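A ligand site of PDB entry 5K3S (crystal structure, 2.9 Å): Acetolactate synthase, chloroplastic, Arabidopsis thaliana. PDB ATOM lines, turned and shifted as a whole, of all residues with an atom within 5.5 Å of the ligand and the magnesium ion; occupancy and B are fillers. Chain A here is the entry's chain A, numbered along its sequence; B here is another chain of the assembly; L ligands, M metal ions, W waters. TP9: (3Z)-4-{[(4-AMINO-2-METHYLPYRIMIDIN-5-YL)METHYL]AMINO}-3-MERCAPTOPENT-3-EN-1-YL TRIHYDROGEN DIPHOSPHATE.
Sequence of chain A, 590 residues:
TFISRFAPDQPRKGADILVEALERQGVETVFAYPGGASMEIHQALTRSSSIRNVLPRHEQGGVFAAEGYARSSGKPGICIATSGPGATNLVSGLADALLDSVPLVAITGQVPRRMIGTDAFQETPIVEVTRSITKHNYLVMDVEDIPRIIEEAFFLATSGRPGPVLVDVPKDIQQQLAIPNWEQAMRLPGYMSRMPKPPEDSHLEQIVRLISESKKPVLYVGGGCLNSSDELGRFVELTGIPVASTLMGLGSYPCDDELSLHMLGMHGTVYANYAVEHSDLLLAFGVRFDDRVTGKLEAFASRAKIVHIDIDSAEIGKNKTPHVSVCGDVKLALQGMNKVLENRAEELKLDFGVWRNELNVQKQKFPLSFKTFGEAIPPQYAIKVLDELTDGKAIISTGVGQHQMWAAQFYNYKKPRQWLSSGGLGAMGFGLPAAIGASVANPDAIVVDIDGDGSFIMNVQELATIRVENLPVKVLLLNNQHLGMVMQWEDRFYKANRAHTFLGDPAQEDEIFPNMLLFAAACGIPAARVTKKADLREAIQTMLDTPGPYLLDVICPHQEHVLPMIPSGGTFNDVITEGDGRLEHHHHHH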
ATOM      1  N   VAL A 400     -23.959  16.501  -7.075  1.00  0.00           N
ATOM      2  CA  VAL A 400     -24.247  17.598  -7.981  1.00  0.00           C
ATOM      3  C   VAL A 400     -25.211  18.594  -7.342  1.00  0.00           C
ATOM      4  O   VAL A 400     -26.251  18.209  -6.798  1.00  0.00           O
ATOM      5  CB  VAL A 400     -24.832  17.100  -9.314  1.00  0.00           C
ATOM      6  CG1 VAL A 400     -25.313  18.258 -10.171  1.00  0.00           C
ATOM      7  CG2 VAL A 400     -23.799  16.274 -10.063  1.00  0.00           C
ATOM      8  N   GLY A 401     -24.857  19.870  -7.393  1.00  0.00           N
ATOM      9  CA  GLY A 401     -25.694  20.923  -6.833  1.00  0.00           C
ATOM     10  C   GLY A 401     -24.905  22.066  -6.240  1.00  0.00           C
ATOM     11  O   GLY A 401     -23.781  22.339  -6.672  1.00  0.00           O
ATOM     12  N   GLN A 402     -25.486  22.727  -5.257  1.00  0.00           N
ATOM     13  CA  GLN A 402     -24.832  23.833  -4.575  1.00  0.00           C
ATOM     14  C   GLN A 402     -23.538  23.390  -3.893  1.00  0.00           C
ATOM     15  O   GLN A 402     -22.520  24.073  -3.978  1.00  0.00           O
ATOM     16  CB  GLN A 402     -25.774  24.469  -3.544  1.00  0.00           C
ATOM     17  CG  GLN A 402     -26.923  25.246  -4.136  1.00  0.00           C
ATOM     18  CD  GLN A 402     -27.787  25.890  -3.074  1.00  0.00           C
ATOM     19  OE1 GLN A 402     -27.932  25.369  -1.974  1.00  0.00           O
ATOM     20  NE2 GLN A 402     -28.378  27.042  -3.402  1.00  0.00           N
ATOM     21  N   HIS A 403     -23.601  22.246  -3.220  1.00  0.00           N
ATOM     22  CA  HIS A 403     -22.455  21.709  -2.500  1.00  0.00           C
ATOM     23  C   HIS A 403     -21.313  21.394  -3.460  1.00  0.00           C
ATOM     24  O   HIS A 403     -20.135  21.486  -3.091  1.00  0.00           O
ATOM     25  CB  HIS A 403     -22.843  20.449  -1.719  1.00  0.00           C
ATOM     26  CG  HIS A 403     -23.134  19.269  -2.587  1.00  0.00           C
ATOM     27  ND1 HIS A 403     -24.336  19.105  -3.256  1.00  0.00           N
ATOM     28  CD2 HIS A 403     -22.377  18.194  -2.908  1.00  0.00           C
ATOM     29  CE1 HIS A 403     -24.297  17.978  -3.942  1.00  0.00           C
ATOM     30  NE2 HIS A 403     -23.125  17.405  -3.752  1.00  0.00           N
ATOM     31  N   GLN A 404     -21.660  21.025  -4.692  1.00  0.00           N
ATOM     32  CA  GLN A 404     -20.665  20.715  -5.713  1.00  0.00           C
ATOM     33  C   GLN A 404     -19.863  21.960  -6.081  1.00  0.00           C
ATOM     34  O   GLN A 404     -18.638  21.896  -6.241  1.00  0.00           O
ATOM     35  CB  GLN A 404     -21.335  20.131  -6.946  1.00  0.00           C
ATOM     36  CG  GLN A 404     -20.367  19.749  -8.058  1.00  0.00           C
ATOM     37  CD  GLN A 404     -21.075  19.398  -9.352  1.00  0.00           C
ATOM     38  OE1 GLN A 404     -22.258  19.716  -9.532  1.00  0.00           O
ATOM     39  NE2 GLN A 404     -20.374  18.731 -10.255  1.00  0.00           N
ATOM     40  N   TRP A 406     -19.506  24.806  -4.257  1.00  0.00           N
ATOM     41  CA  TRP A 406     -18.735  25.264  -3.102  1.00  0.00           C
ATOM     42  C   TRP A 406     -17.511  24.387  -2.880  1.00  0.00           C
ATOM     43  O   TRP A 406     -16.473  24.881  -2.433  1.00  0.00           O
ATOM     44  CB  TRP A 406     -19.622  25.286  -1.849  1.00  0.00           C
ATOM     45  CG  TRP A 406     -20.687  26.328  -1.900  1.00  0.00           C
ATOM     46  CD1 TRP A 406     -20.584  27.586  -2.424  1.00  0.00           C
ATOM     47  CD2 TRP A 406     -22.033  26.201  -1.430  1.00  0.00           C
ATOM     48  NE1 TRP A 406     -21.774  28.259  -2.285  1.00  0.00           N
ATOM     49  CE2 TRP A 406     -22.689  27.430  -1.689  1.00  0.00           C
ATOM     50  CE3 TRP A 406     -22.762  25.176  -0.813  1.00  0.00           C
ATOM     51  CZ2 TRP A 406     -24.016  27.650  -1.340  1.00  0.00           C
ATOM     52  CZ3 TRP A 406     -24.082  25.403  -0.474  1.00  0.00           C
ATOM     53  CH2 TRP A 406     -24.695  26.633  -0.742  1.00  0.00           C
ATOM     54  N   LEU A 425     -22.475  15.643 -17.641  1.00  0.00           N
ATOM     55  CA  LEU A 425     -23.807  15.098 -17.390  1.00  0.00           C
ATOM     56  C   LEU A 425     -24.375  15.647 -16.086  1.00  0.00           C
ATOM     57  O   LEU A 425     -25.580  15.860 -15.966  1.00  0.00           O
ATOM     58  CB  LEU A 425     -23.755  13.564 -17.345  1.00  0.00           C
ATOM     59  CG  LEU A 425     -25.104  12.842 -17.333  1.00  0.00           C
ATOM     60  CD1 LEU A 425     -25.854  13.077 -18.640  1.00  0.00           C
ATOM     61  CD2 LEU A 425     -24.905  11.346 -17.087  1.00  0.00           C
ATOM     62  N   GLY A 426     -23.501  15.865 -15.110  1.00  0.00           N
ATOM     63  CA  GLY A 426     -23.913  16.360 -13.805  1.00  0.00           C
ATOM     64  C   GLY A 426     -24.897  15.418 -13.139  1.00  0.00           C
ATOM     65  O   GLY A 426     -26.035  15.788 -12.849  1.00  0.00           O
ATOM     66  N   ALA A 427     -24.447  14.193 -12.882  1.00  0.00           N
ATOM     67  CA  ALA A 427     -25.309  13.160 -12.326  1.00  0.00           C
ATOM     68  C   ALA A 427     -25.235  13.095 -10.805  1.00  0.00           C
ATOM     69  O   ALA A 427     -24.156  12.918 -10.246  1.00  0.00           O
ATOM     70  CB  ALA A 427     -24.964  11.804 -12.929  1.00  0.00           C
ATOM     71  N   MET A 428     -26.381  13.247 -10.154  1.00  0.00           N
ATOM     72  CA  MET A 428     -26.468  13.088  -8.704  1.00  0.00           C
ATOM     73  C   MET A 428     -26.165  11.643  -8.307  1.00  0.00           C
ATOM     74  O   MET A 428     -26.290  10.733  -9.115  1.00  0.00           O
ATOM     75  CB  MET A 428     -27.841  13.505  -8.196  1.00  0.00           C
ATOM     76  CG  MET A 428     -28.119  14.994  -8.293  1.00  0.00           C
ATOM     77  SD  MET A 428     -29.831  15.393  -7.887  1.00  0.00           S
ATOM     78  CE  MET A 428     -29.956  14.683  -6.246  1.00  0.00           C
ATOM     79  N   GLY A 452     -24.405  16.254  -1.148  1.00  0.00           N
ATOM     80  CA  GLY A 452     -25.646  16.920  -0.769  1.00  0.00           C
ATOM     81  C   GLY A 452     -26.642  15.892  -0.294  1.00  0.00           C
ATOM     82  O   GLY A 452     -26.541  14.718  -0.660  1.00  0.00           O
ATOM     83  N   ASP A 453     -27.601  16.308   0.517  1.00  0.00           N
ATOM     84  CA  ASP A 453     -28.564  15.373   1.113  1.00  0.00           C
ATOM     85  C   ASP A 453     -29.425  14.681   0.068  1.00  0.00           C
ATOM     86  O   ASP A 453     -29.909  13.573   0.298  1.00  0.00           O
ATOM     87  CB  ASP A 453     -29.457  16.101   2.124  1.00  0.00           C
ATOM     88  CG  ASP A 453     -30.180  17.286   1.514  1.00  0.00           C
ATOM     89  OD1 ASP A 453     -29.566  18.019   0.717  1.00  0.00           O
ATOM     90  OD2 ASP A 453     -31.372  17.472   1.844  1.00  0.00           O
ATOM     91  N   GLY A 454     -29.607  15.326  -1.075  1.00  0.00           N
ATOM     92  CA  GLY A 454     -30.356  14.734  -2.169  1.00  0.00           C
ATOM     93  C   GLY A 454     -29.497  13.758  -2.960  1.00  0.00           C
ATOM     94  O   GLY A 454     -29.949  12.663  -3.310  1.00  0.00           O
ATOM     95  N   SER A 455     -28.262  14.160  -3.241  1.00  0.00           N
ATOM     96  CA  SER A 455     -27.341  13.333  -4.012  1.00  0.00           C
ATOM     97  C   SER A 455     -26.888  12.118  -3.214  1.00  0.00           C
ATOM     98  O   SER A 455     -26.730  11.029  -3.770  1.00  0.00           O
ATOM     99  CB  SER A 455     -26.138  14.159  -4.455  1.00  0.00           C
ATOM    100  OG  SER A 455     -26.534  15.276  -5.231  1.00  0.00           O
ATOM    101  N   PHE A 456     -26.688  12.308  -1.923  1.00  0.00           N
ATOM    102  CA  PHE A 456     -26.181  11.249  -1.056  1.00  0.00           C
ATOM    103  C   PHE A 456     -27.166  10.085  -0.920  1.00  0.00           C
ATOM    104  O   PHE A 456     -26.750   8.923  -0.913  1.00  0.00           O
ATOM    105  CB  PHE A 456     -25.859  11.808   0.335  1.00  0.00           C
ATOM    106  CG  PHE A 456     -25.395  10.777   1.322  1.00  0.00           C
ATOM    107  CD1 PHE A 456     -24.115  10.240   1.233  1.00  0.00           C
ATOM    108  CD2 PHE A 456     -26.232  10.332   2.327  1.00  0.00           C
ATOM    109  CE1 PHE A 456     -23.687   9.286   2.140  1.00  0.00           C
ATOM    110  CE2 PHE A 456     -25.818   9.378   3.233  1.00  0.00           C
ATOM    111  CZ  PHE A 456     -24.539   8.855   3.144  1.00  0.00           C
ATOM    112  N   MET A 458     -29.443   9.035  -2.984  1.00  0.00           N
ATOM    113  CA  MET A 458     -29.716   8.313  -4.224  1.00  0.00           C
ATOM    114  C   MET A 458     -28.979   6.978  -4.294  1.00  0.00           C
ATOM    115  O   MET A 458     -29.558   5.966  -4.696  1.00  0.00           O
ATOM    116  CB  MET A 458     -29.334   9.162  -5.444  1.00  0.00           C
ATOM    117  CG  MET A 458     -30.382  10.203  -5.815  1.00  0.00           C
ATOM    118  SD  MET A 458     -30.220  10.737  -7.536  1.00  0.00           S
ATOM    119  CE  MET A 458     -31.686  11.738  -7.720  1.00  0.00           C
ATOM    120  N   LEU A 478     -23.159  17.994   3.377  1.00  0.00           N
ATOM    121  CA  LEU A 478     -23.712  19.331   3.538  1.00  0.00           C
ATOM    122  C   LEU A 478     -25.231  19.264   3.417  1.00  0.00           C
ATOM    123  O   LEU A 478     -25.774  19.241   2.312  1.00  0.00           O
ATOM    124  CB  LEU A 478     -23.135  20.296   2.510  1.00  0.00           C
ATOM    125  CG  LEU A 478     -21.610  20.455   2.521  1.00  0.00           C
ATOM    126  CD1 LEU A 478     -21.169  21.553   1.571  1.00  0.00           C
ATOM    127  CD2 LEU A 478     -21.107  20.713   3.934  1.00  0.00           C
ATOM    128  N   ASN A 480     -28.848  20.660   3.594  1.00  0.00           N
ATOM    129  CA  ASN A 480     -29.681  21.852   3.564  1.00  0.00           C
ATOM    130  C   ASN A 480     -31.169  21.503   3.463  1.00  0.00           C
ATOM    131  O   ASN A 480     -31.997  22.384   3.244  1.00  0.00           O
ATOM    132  CB  ASN A 480     -29.280  22.766   2.404  1.00  0.00           C
ATOM    133  CG  ASN A 480     -29.247  22.040   1.067  1.00  0.00           C
ATOM    134  OD1 ASN A 480     -29.742  20.917   0.936  1.00  0.00           O
ATOM    135  ND2 ASN A 480     -28.674  22.687   0.059  1.00  0.00           N
ATOM    136  N   GLN A 481     -31.473  20.220   3.595  1.00  0.00           N
ATOM    137  CA  GLN A 481     -32.847  19.717   3.566  1.00  0.00           C
ATOM    138  C   GLN A 481     -33.569  20.051   2.259  1.00  0.00           C
ATOM    139  O   GLN A 481     -34.798  20.023   2.200  1.00  0.00           O
ATOM    140  CB  GLN A 481     -33.647  20.256   4.748  1.00  0.00           C
ATOM    141  CG  GLN A 481     -33.136  19.806   6.114  1.00  0.00           C
ATOM    142  CD  GLN A 481     -33.433  18.347   6.386  1.00  0.00           C
ATOM    143  OE1 GLN A 481     -34.473  18.005   6.939  1.00  0.00           O
ATOM    144  NE2 GLN A 481     -32.501  17.465   6.006  1.00  0.00           N
ATOM    145  N   HIS A 482     -32.807  20.360   1.224  1.00  0.00           N
ATOM    146  CA  HIS A 482     -33.382  20.788  -0.052  1.00  0.00           C
ATOM    147  C   HIS A 482     -32.583  20.305  -1.244  1.00  0.00           C
ATOM    148  O   HIS A 482     -31.454  19.830  -1.114  1.00  0.00           O
ATOM    149  CB  HIS A 482     -33.484  22.314  -0.117  1.00  0.00           C
ATOM    150  CG  HIS A 482     -34.621  22.891   0.682  1.00  0.00           C
ATOM    151  ND1 HIS A 482     -34.569  23.030   2.052  1.00  0.00           N
ATOM    152  CD2 HIS A 482     -35.825  23.357   0.301  1.00  0.00           C
ATOM    153  CE1 HIS A 482     -35.696  23.570   2.482  1.00  0.00           C
ATOM    154  NE2 HIS A 482     -36.482  23.770   1.435  1.00  0.00           N
ATOM    155  N   LEU A 483     -33.190  20.415  -2.429  1.00  0.00           N
ATOM    156  CA  LEU A 483     -32.451  20.299  -3.673  1.00  0.00           C
ATOM    157  C   LEU A 483     -31.933  21.697  -4.023  1.00  0.00           C
ATOM    158  O   LEU A 483     -32.457  22.367  -4.910  1.00  0.00           O
ATOM    159  CB  LEU A 483     -33.341  19.748  -4.788  1.00  0.00           C
ATOM    160  CG  LEU A 483     -33.907  18.342  -4.568  1.00  0.00           C
ATOM    161  CD1 LEU A 483     -34.877  17.967  -5.665  1.00  0.00           C
ATOM    162  CD2 LEU A 483     -32.786  17.315  -4.476  1.00  0.00           C
ATOM    163  N   GLY A 484     -30.897  22.107  -3.297  1.00  0.00           N
ATOM    164  CA  GLY A 484     -30.418  23.484  -3.287  1.00  0.00           C
ATOM    165  C   GLY A 484     -30.281  24.195  -4.618  1.00  0.00           C
ATOM    166  O   GLY A 484     -30.724  25.343  -4.745  1.00  0.00           O
ATOM    167  N   MET A 485     -29.665  23.542  -5.592  1.00  0.00           N
ATOM    168  CA  MET A 485     -29.414  24.156  -6.892  1.00  0.00           C
ATOM    169  C   MET A 485     -30.715  24.563  -7.583  1.00  0.00           C
ATOM    170  O   MET A 485     -30.830  25.670  -8.087  1.00  0.00           O
ATOM    171  CB  MET A 485     -28.619  23.200  -7.782  1.00  0.00           C
ATOM    172  CG  MET A 485     -28.121  23.824  -9.091  1.00  0.00           C
ATOM    173  SD  MET A 485     -26.706  24.915  -8.873  1.00  0.00           S
ATOM    174  CE  MET A 485     -27.496  26.512  -8.694  1.00  0.00           C
ATOM    175  N   VAL A 486     -31.687  23.654  -7.598  1.00  0.00           N
ATOM    176  CA  VAL A 486     -32.987  23.934  -8.179  1.00  0.00           C
ATOM    177  C   VAL A 486     -33.720  24.982  -7.338  1.00  0.00           C
ATOM    178  O   VAL A 486     -34.397  25.857  -7.866  1.00  0.00           O
ATOM    179  CB  VAL A 486     -33.856  22.658  -8.281  1.00  0.00           C
ATOM    180  CG1 VAL A 486     -35.205  22.974  -8.913  1.00  0.00           C
ATOM    181  CG2 VAL A 486     -33.124  21.596  -9.082  1.00  0.00           C
ATOM    182  N   LEU A 503     -36.797  18.249   0.840  1.00  0.00           N
ATOM    183  CA  LEU A 503     -36.507  16.831   0.997  1.00  0.00           C
ATOM    184  C   LEU A 503     -36.851  16.295   2.386  1.00  0.00           C
ATOM    185  O   LEU A 503     -36.740  15.094   2.640  1.00  0.00           O
ATOM    186  CB  LEU A 503     -35.038  16.557   0.699  1.00  0.00           C
ATOM    187  CG  LEU A 503     -34.577  16.869  -0.719  1.00  0.00           C
ATOM    188  CD1 LEU A 503     -33.081  16.609  -0.866  1.00  0.00           C
ATOM    189  CD2 LEU A 503     -35.359  16.044  -1.732  1.00  0.00           C
ATOM    190  N   TYR B  33     -39.420  14.095 -10.588  1.00  0.00           N
ATOM    191  CA  TYR B  33     -38.221  14.543  -9.870  1.00  0.00           C
ATOM    192  C   TYR B  33     -37.614  15.728 -10.609  1.00  0.00           C
ATOM    193  O   TYR B  33     -37.151  15.588 -11.745  1.00  0.00           O
ATOM    194  CB  TYR B  33     -37.219  13.394  -9.749  1.00  0.00           C
ATOM    195  CG  TYR B  33     -36.155  13.622  -8.691  1.00  0.00           C
ATOM    196  CD1 TYR B  33     -35.016  14.355  -8.974  1.00  0.00           C
ATOM    197  CD2 TYR B  33     -36.301  13.101  -7.410  1.00  0.00           C
ATOM    198  CE1 TYR B  33     -34.042  14.560  -8.008  1.00  0.00           C
ATOM    199  CE2 TYR B  33     -35.342  13.306  -6.444  1.00  0.00           C
ATOM    200  CZ  TYR B  33     -34.209  14.032  -6.747  1.00  0.00           C
ATOM    201  OH  TYR B  33     -33.250  14.237  -5.780  1.00  0.00           O
ATOM    202  N   PRO B  34     -37.604  16.904  -9.963  1.00  0.00           N
ATOM    203  CA  PRO B  34     -37.238  18.172 -10.614  1.00  0.00           C
ATOM    204  C   PRO B  34     -35.772  18.265 -11.033  1.00  0.00           C
ATOM    205  O   PRO B  34     -34.906  17.597 -10.484  1.00  0.00           O
ATOM    206  CB  PRO B  34     -37.534  19.212  -9.529  1.00  0.00           C
ATOM    207  CG  PRO B  34     -37.408  18.467  -8.256  1.00  0.00           C
ATOM    208  CD  PRO B  34     -37.914  17.089  -8.536  1.00  0.00           C
ATOM    209  N   GLY B  35     -35.527  19.106 -12.033  1.00  0.00           N
ATOM    210  CA  GLY B  35     -34.197  19.388 -12.514  1.00  0.00           C
ATOM    211  C   GLY B  35     -34.232  20.629 -13.388  1.00  0.00           C
ATOM    212  O   GLY B  35     -35.316  21.090 -13.758  1.00  0.00           O
ATOM    213  N   GLY B  36     -33.069  21.172 -13.711  1.00  0.00           N
ATOM    214  CA  GLY B  36     -32.971  22.408 -14.454  1.00  0.00           C
ATOM    215  C   GLY B  36     -33.739  22.452 -15.760  1.00  0.00           C
ATOM    216  O   GLY B  36     -34.307  23.484 -16.128  1.00  0.00           O
ATOM    217  N   GLU B  59     -35.010   8.717  -9.747  1.00  0.00           N
ATOM    218  CA  GLU B  59     -35.890   8.604 -10.913  1.00  0.00           C
ATOM    219  C   GLU B  59     -36.261   7.149 -11.222  1.00  0.00           C
ATOM    220  O   GLU B  59     -37.343   6.881 -11.729  1.00  0.00           O
ATOM    221  CB  GLU B  59     -35.252   9.244 -12.140  1.00  0.00           C
ATOM    222  CG  GLU B  59     -35.234  10.764 -12.115  1.00  0.00           C
ATOM    223  CD  GLU B  59     -33.979  11.325 -11.467  1.00  0.00           C
ATOM    224  OE1 GLU B  59     -33.197  10.530 -10.888  1.00  0.00           O
ATOM    225  OE2 GLU B  59     -33.773  12.551 -11.549  1.00  0.00           O
ATOM    226  N   THR B  82     -35.845  15.124 -15.374  1.00  0.00           N
ATOM    227  CA  THR B  82     -35.137  16.170 -16.091  1.00  0.00           C
ATOM    228  C   THR B  82     -34.238  15.561 -17.163  1.00  0.00           C
ATOM    229  O   THR B  82     -34.194  14.345 -17.328  1.00  0.00           O
ATOM    230  CB  THR B  82     -34.284  17.038 -15.147  1.00  0.00           C
ATOM    231  OG1 THR B  82     -33.761  18.166 -15.867  1.00  0.00           O
ATOM    232  CG2 THR B  82     -33.134  16.232 -14.556  1.00  0.00           C
ATOM    233  N   PRO B  85     -28.965  13.019 -16.754  1.00  0.00           N
ATOM    234  CA  PRO B  85     -28.919  12.005 -15.690  1.00  0.00           C
ATOM    235  C   PRO B  85     -30.298  11.616 -15.180  1.00  0.00           C
ATOM    236  O   PRO B  85     -30.500  10.484 -14.758  1.00  0.00           O
ATOM    237  CB  PRO B  85     -28.101  12.697 -14.586  1.00  0.00           C
ATOM    238  CG  PRO B  85     -28.299  14.150 -14.832  1.00  0.00           C
ATOM    239  CD  PRO B  85     -28.360  14.286 -16.323  1.00  0.00           C
ATOM    240  N   GLY B  86     -31.241  12.553 -15.230  1.00  0.00           N
ATOM    241  CA  GLY B  86     -32.599  12.270 -14.829  1.00  0.00           C
ATOM    242  C   GLY B  86     -33.252  11.291 -15.791  1.00  0.00           C
ATOM    243  O   GLY B  86     -33.917  10.345 -15.384  1.00  0.00           O
ATOM    244  N   ASN B  89     -31.840   7.658 -15.759  1.00  0.00           N
ATOM    245  CA  ASN B  89     -32.243   6.901 -14.580  1.00  0.00           C
ATOM    246  C   ASN B  89     -33.621   6.248 -14.769  1.00  0.00           C
ATOM    247  O   ASN B  89     -34.071   5.482 -13.910  1.00  0.00           O
ATOM    248  CB  ASN B  89     -32.263   7.796 -13.343  1.00  0.00           C
ATOM    249  CG  ASN B  89     -30.876   7.962 -12.732  1.00  0.00           C
ATOM    250  OD1 ASN B  89     -29.967   7.186 -13.013  1.00  0.00           O
ATOM    251  ND2 ASN B  89     -30.725   8.970 -11.884  1.00  0.00           N
ATOM    252  N   GLN B 122     -25.981  18.617 -19.368  1.00  0.00           N
ATOM    253  CA  GLN B 122     -26.983  17.596 -19.053  1.00  0.00           C
ATOM    254  C   GLN B 122     -27.789  17.172 -20.278  1.00  0.00           C
ATOM    255  O   GLN B 122     -28.990  16.961 -20.186  1.00  0.00           O
ATOM    256  CB  GLN B 122     -27.931  18.083 -17.951  1.00  0.00           C
ATOM    257  CG  GLN B 122     -27.238  18.435 -16.647  1.00  0.00           C
ATOM    258  CD  GLN B 122     -28.210  18.555 -15.495  1.00  0.00           C
ATOM    259  OE1 GLN B 122     -27.930  18.095 -14.381  1.00  0.00           O
ATOM    260  NE2 GLN B 122     -29.360  19.163 -15.746  1.00  0.00           N
HETATM  261  N1' TP9 L   1     -31.231  13.727 -11.033  1.00  0.00           N
HETATM  262  C2' TP9 L   1     -29.947  13.507 -11.233  1.00  0.00           C
HETATM  263  CM2 TP9 L   1     -29.457  12.077 -11.224  1.00  0.00           C
HETATM  264  N3' TP9 L   1     -29.079  14.478 -11.429  1.00  0.00           N
HETATM  265  C4' TP9 L   1     -29.475  15.760 -11.436  1.00  0.00           C
HETATM  266  N4' TP9 L   1     -28.517  16.796 -11.652  1.00  0.00           N
HETATM  267  C5' TP9 L   1     -30.838  16.057 -11.237  1.00  0.00           C
HETATM  268  C6' TP9 L   1     -31.711  14.980 -11.031  1.00  0.00           C
HETATM  269  C7' TP9 L   1     -31.370  17.472 -11.236  1.00  0.00           C
HETATM  270  N3  TP9 L   1     -30.594  18.332 -10.413  1.00  0.00           N
HETATM  271  S1  TP9 L   1     -28.396  19.671  -8.630  1.00  0.00           S
HETATM  272  C5  TP9 L   1     -30.005  19.089  -8.170  1.00  0.00           C
HETATM  273  C4  TP9 L   1     -30.876  18.531  -9.035  1.00  0.00           C
HETATM  274  CM4 TP9 L   1     -32.252  18.029  -8.675  1.00  0.00           C
HETATM  275  C6  TP9 L   1     -30.245  19.331  -6.693  1.00  0.00           C
HETATM  276  C7  TP9 L   1     -29.519  18.324  -5.814  1.00  0.00           C
HETATM  277  O7  TP9 L   1     -29.507  18.823  -4.496  1.00  0.00           O
HETATM  278  PA  TP9 L   1     -28.455  18.237  -3.466  1.00  0.00           P
HETATM  279  O1A TP9 L   1     -27.941  16.898  -3.967  1.00  0.00           O
HETATM  280  O2A TP9 L   1     -29.099  18.050  -2.120  1.00  0.00           O
HETATM  281  O3A TP9 L   1     -27.258  19.248  -3.339  1.00  0.00           O
HETATM  282  PB  TP9 L   1     -27.455  20.782  -2.986  1.00  0.00           P
HETATM  283  O1B TP9 L   1     -27.574  21.575  -4.269  1.00  0.00           O
HETATM  284  O2B TP9 L   1     -28.722  20.954  -2.176  1.00  0.00           O
HETATM  285  O3B TP9 L   1     -26.278  21.278  -2.188  1.00  0.00           O
HETATM  286 MG    MG M   1     -29.404  19.600  -0.677  1.00  0.00          MG
HETATM  287  O   HOH W   1     -27.339  19.718   0.059  1.00  0.00           O
HETATM  288  O   HOH W   2     -29.911  21.109 -11.346  1.00  0.00           O
HETATM  289  O   HOH W   3     -28.035   9.118 -10.534  1.00  0.00           O
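C of Gly 452 touches O2A of the ligand, 3.7 Å away.
Met 458 touches the ligand.
Leu 483 touches the ligand.
Val 486 touches the ligand.
CE1 of Tyr 33 of chain B touches C6' of the ligand (3.8 Å).
Pro 34 of chain B touches the ligand (O to CM4, 3.2 Å).
CA of Gly 35 of chain B touches C7' of the ligand (3.6 Å).
Thr 82 of chain B touches the ligand (CG2 to C7', 3.96 Å).
Pro 85 of chain B touches the ligand.
Asn 89 of chain B touches the ligand (ND2 to CM2, 3.4 Å).
Hydrophobic or aromatic side chains that line the ligand: Val 400, His 403, Met 428, Met 458, Leu 483, Met 485, Val 486, Tyr 33 of chain B and Pro 85 of chain B.
Of the 35 residues printed, 25 come within 4 Å of the ligand.
Merely in contact with the magnesium ion: Gly 484.
Four residues have an atom within 4 Å of the magnesium ion: Asp 453, Asn 480, His 482 and Gly 484.
The nearest printed residue that does not touch the magnesium ion is Leu 483 (4.3 Å).
The magnesium ion is bound by the backbone carbonyl oxygen of His 482 (2.1 Å), the side-chain amide oxygen of Asn 480 (2.1 Å), the side-chain carboxylate of Asp 453 (2.1 Å), an oxygen (O2B) of the ligand (2.1 Å), an oxygen (O2A) of the ligand (2.1 Å) and water W1 (2.2 Å).
A sulfur (S1) of the ligand lies close to the backbone NH of Gly 401 (3.8 Å).
N of Asp 453 sits close to O2A of the ligand (3.5 Å).
The backbone NH (N) of Gln 402 sits at hydrogen-bond distance from an oxygen (O1B) of the ligand (2.6 Å).
The side-chain amide oxygen (OE1) of Gln 122 of chain B sits at hydrogen-bond distance from a nitrogen (N4') of the ligand, at 3.1 Å.
N3' of the ligand is in hydrogen-bond range of N of Met 428, at 3.2 Å.
N of Ser 455 lies within hydrogen-bond range of O1A of the ligand, at 2.9 Å.
S1 of the ligand sits close to O of Val 400 (3.2 Å).
O1B of the ligand lies within hydrogen-bond range of N of Met 485, at 3.2 Å.
The side-chain hydroxyl (OG) of Ser 455 is in hydrogen-bond range of an oxygen (O1A) of the ligand (2.5 Å).
OE2 of Glu 59 of chain B is in hydrogen-bond range of N1' of the ligand.
The backbone carbonyl oxygen (O) of Gly 426 sits at hydrogen-bond distance from a nitrogen (N4') of the ligand.
N of Gly 454 sits close to O2A of the ligand (3.0 Å).
The backbone NH (N) of His 403 sits at hydrogen-bond distance from an oxygen (O3B) of the ligand, 3.0 Å away.
An oxygen (O3A) of the ligand is in hydrogen-bond range of a ring nitrogen (ND1) of His 403, 2.9 Å away.
The backbone NH (N) of Gly 484 sits close to an oxygen (O2B) of the ligand (2.7 Å).
O of Gly 426 sits close to OE1 of Gln 122 of chain B, 3.4 Å away.
The side-chain amide oxygen (OE1) of Gln 404 lies within hydrogen-bond range of the backbone NH (N) of Gly 401, at 3.4 Å.
The side-chain amide nitrogen (ND2) of Asn 480 is in hydrogen-bond range of the side-chain amide oxygen (OE1) of Gln 402 (3.4 Å).
OE1 of Glu 59 of chain B is in hydrogen-bond range of ND2 of Asn 89 of chain B (3.1 Å).
The side-chain amide nitrogen (ND2) of Asn 89 of chain B sits at hydrogen-bond distance from the backbone carbonyl oxygen (O) of Pro 85 of chain B, 3.3 Å away.
The backbone carbonyl oxygen (O) of Gly 484 is in hydrogen-bond range of the side-chain amide nitrogen (NE2) of Gln 402, 3.2 Å away.
NE2 of His 403 lies within hydrogen-bond range of N of Gly 452 (3.1 Å).
OD2 of Asp 453 sits close to N of Gln 481, at 3.3 Å.
Water W1 lies within hydrogen-bond range of O of Leu 478, O3B of the ligand, ND2 of Asn 480 and N of Asp 453.
Water W3 lies within hydrogen-bond range of O of Met 428 (2.8 Å) and ND2 of Asn 89 of chain B (3.0 Å).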
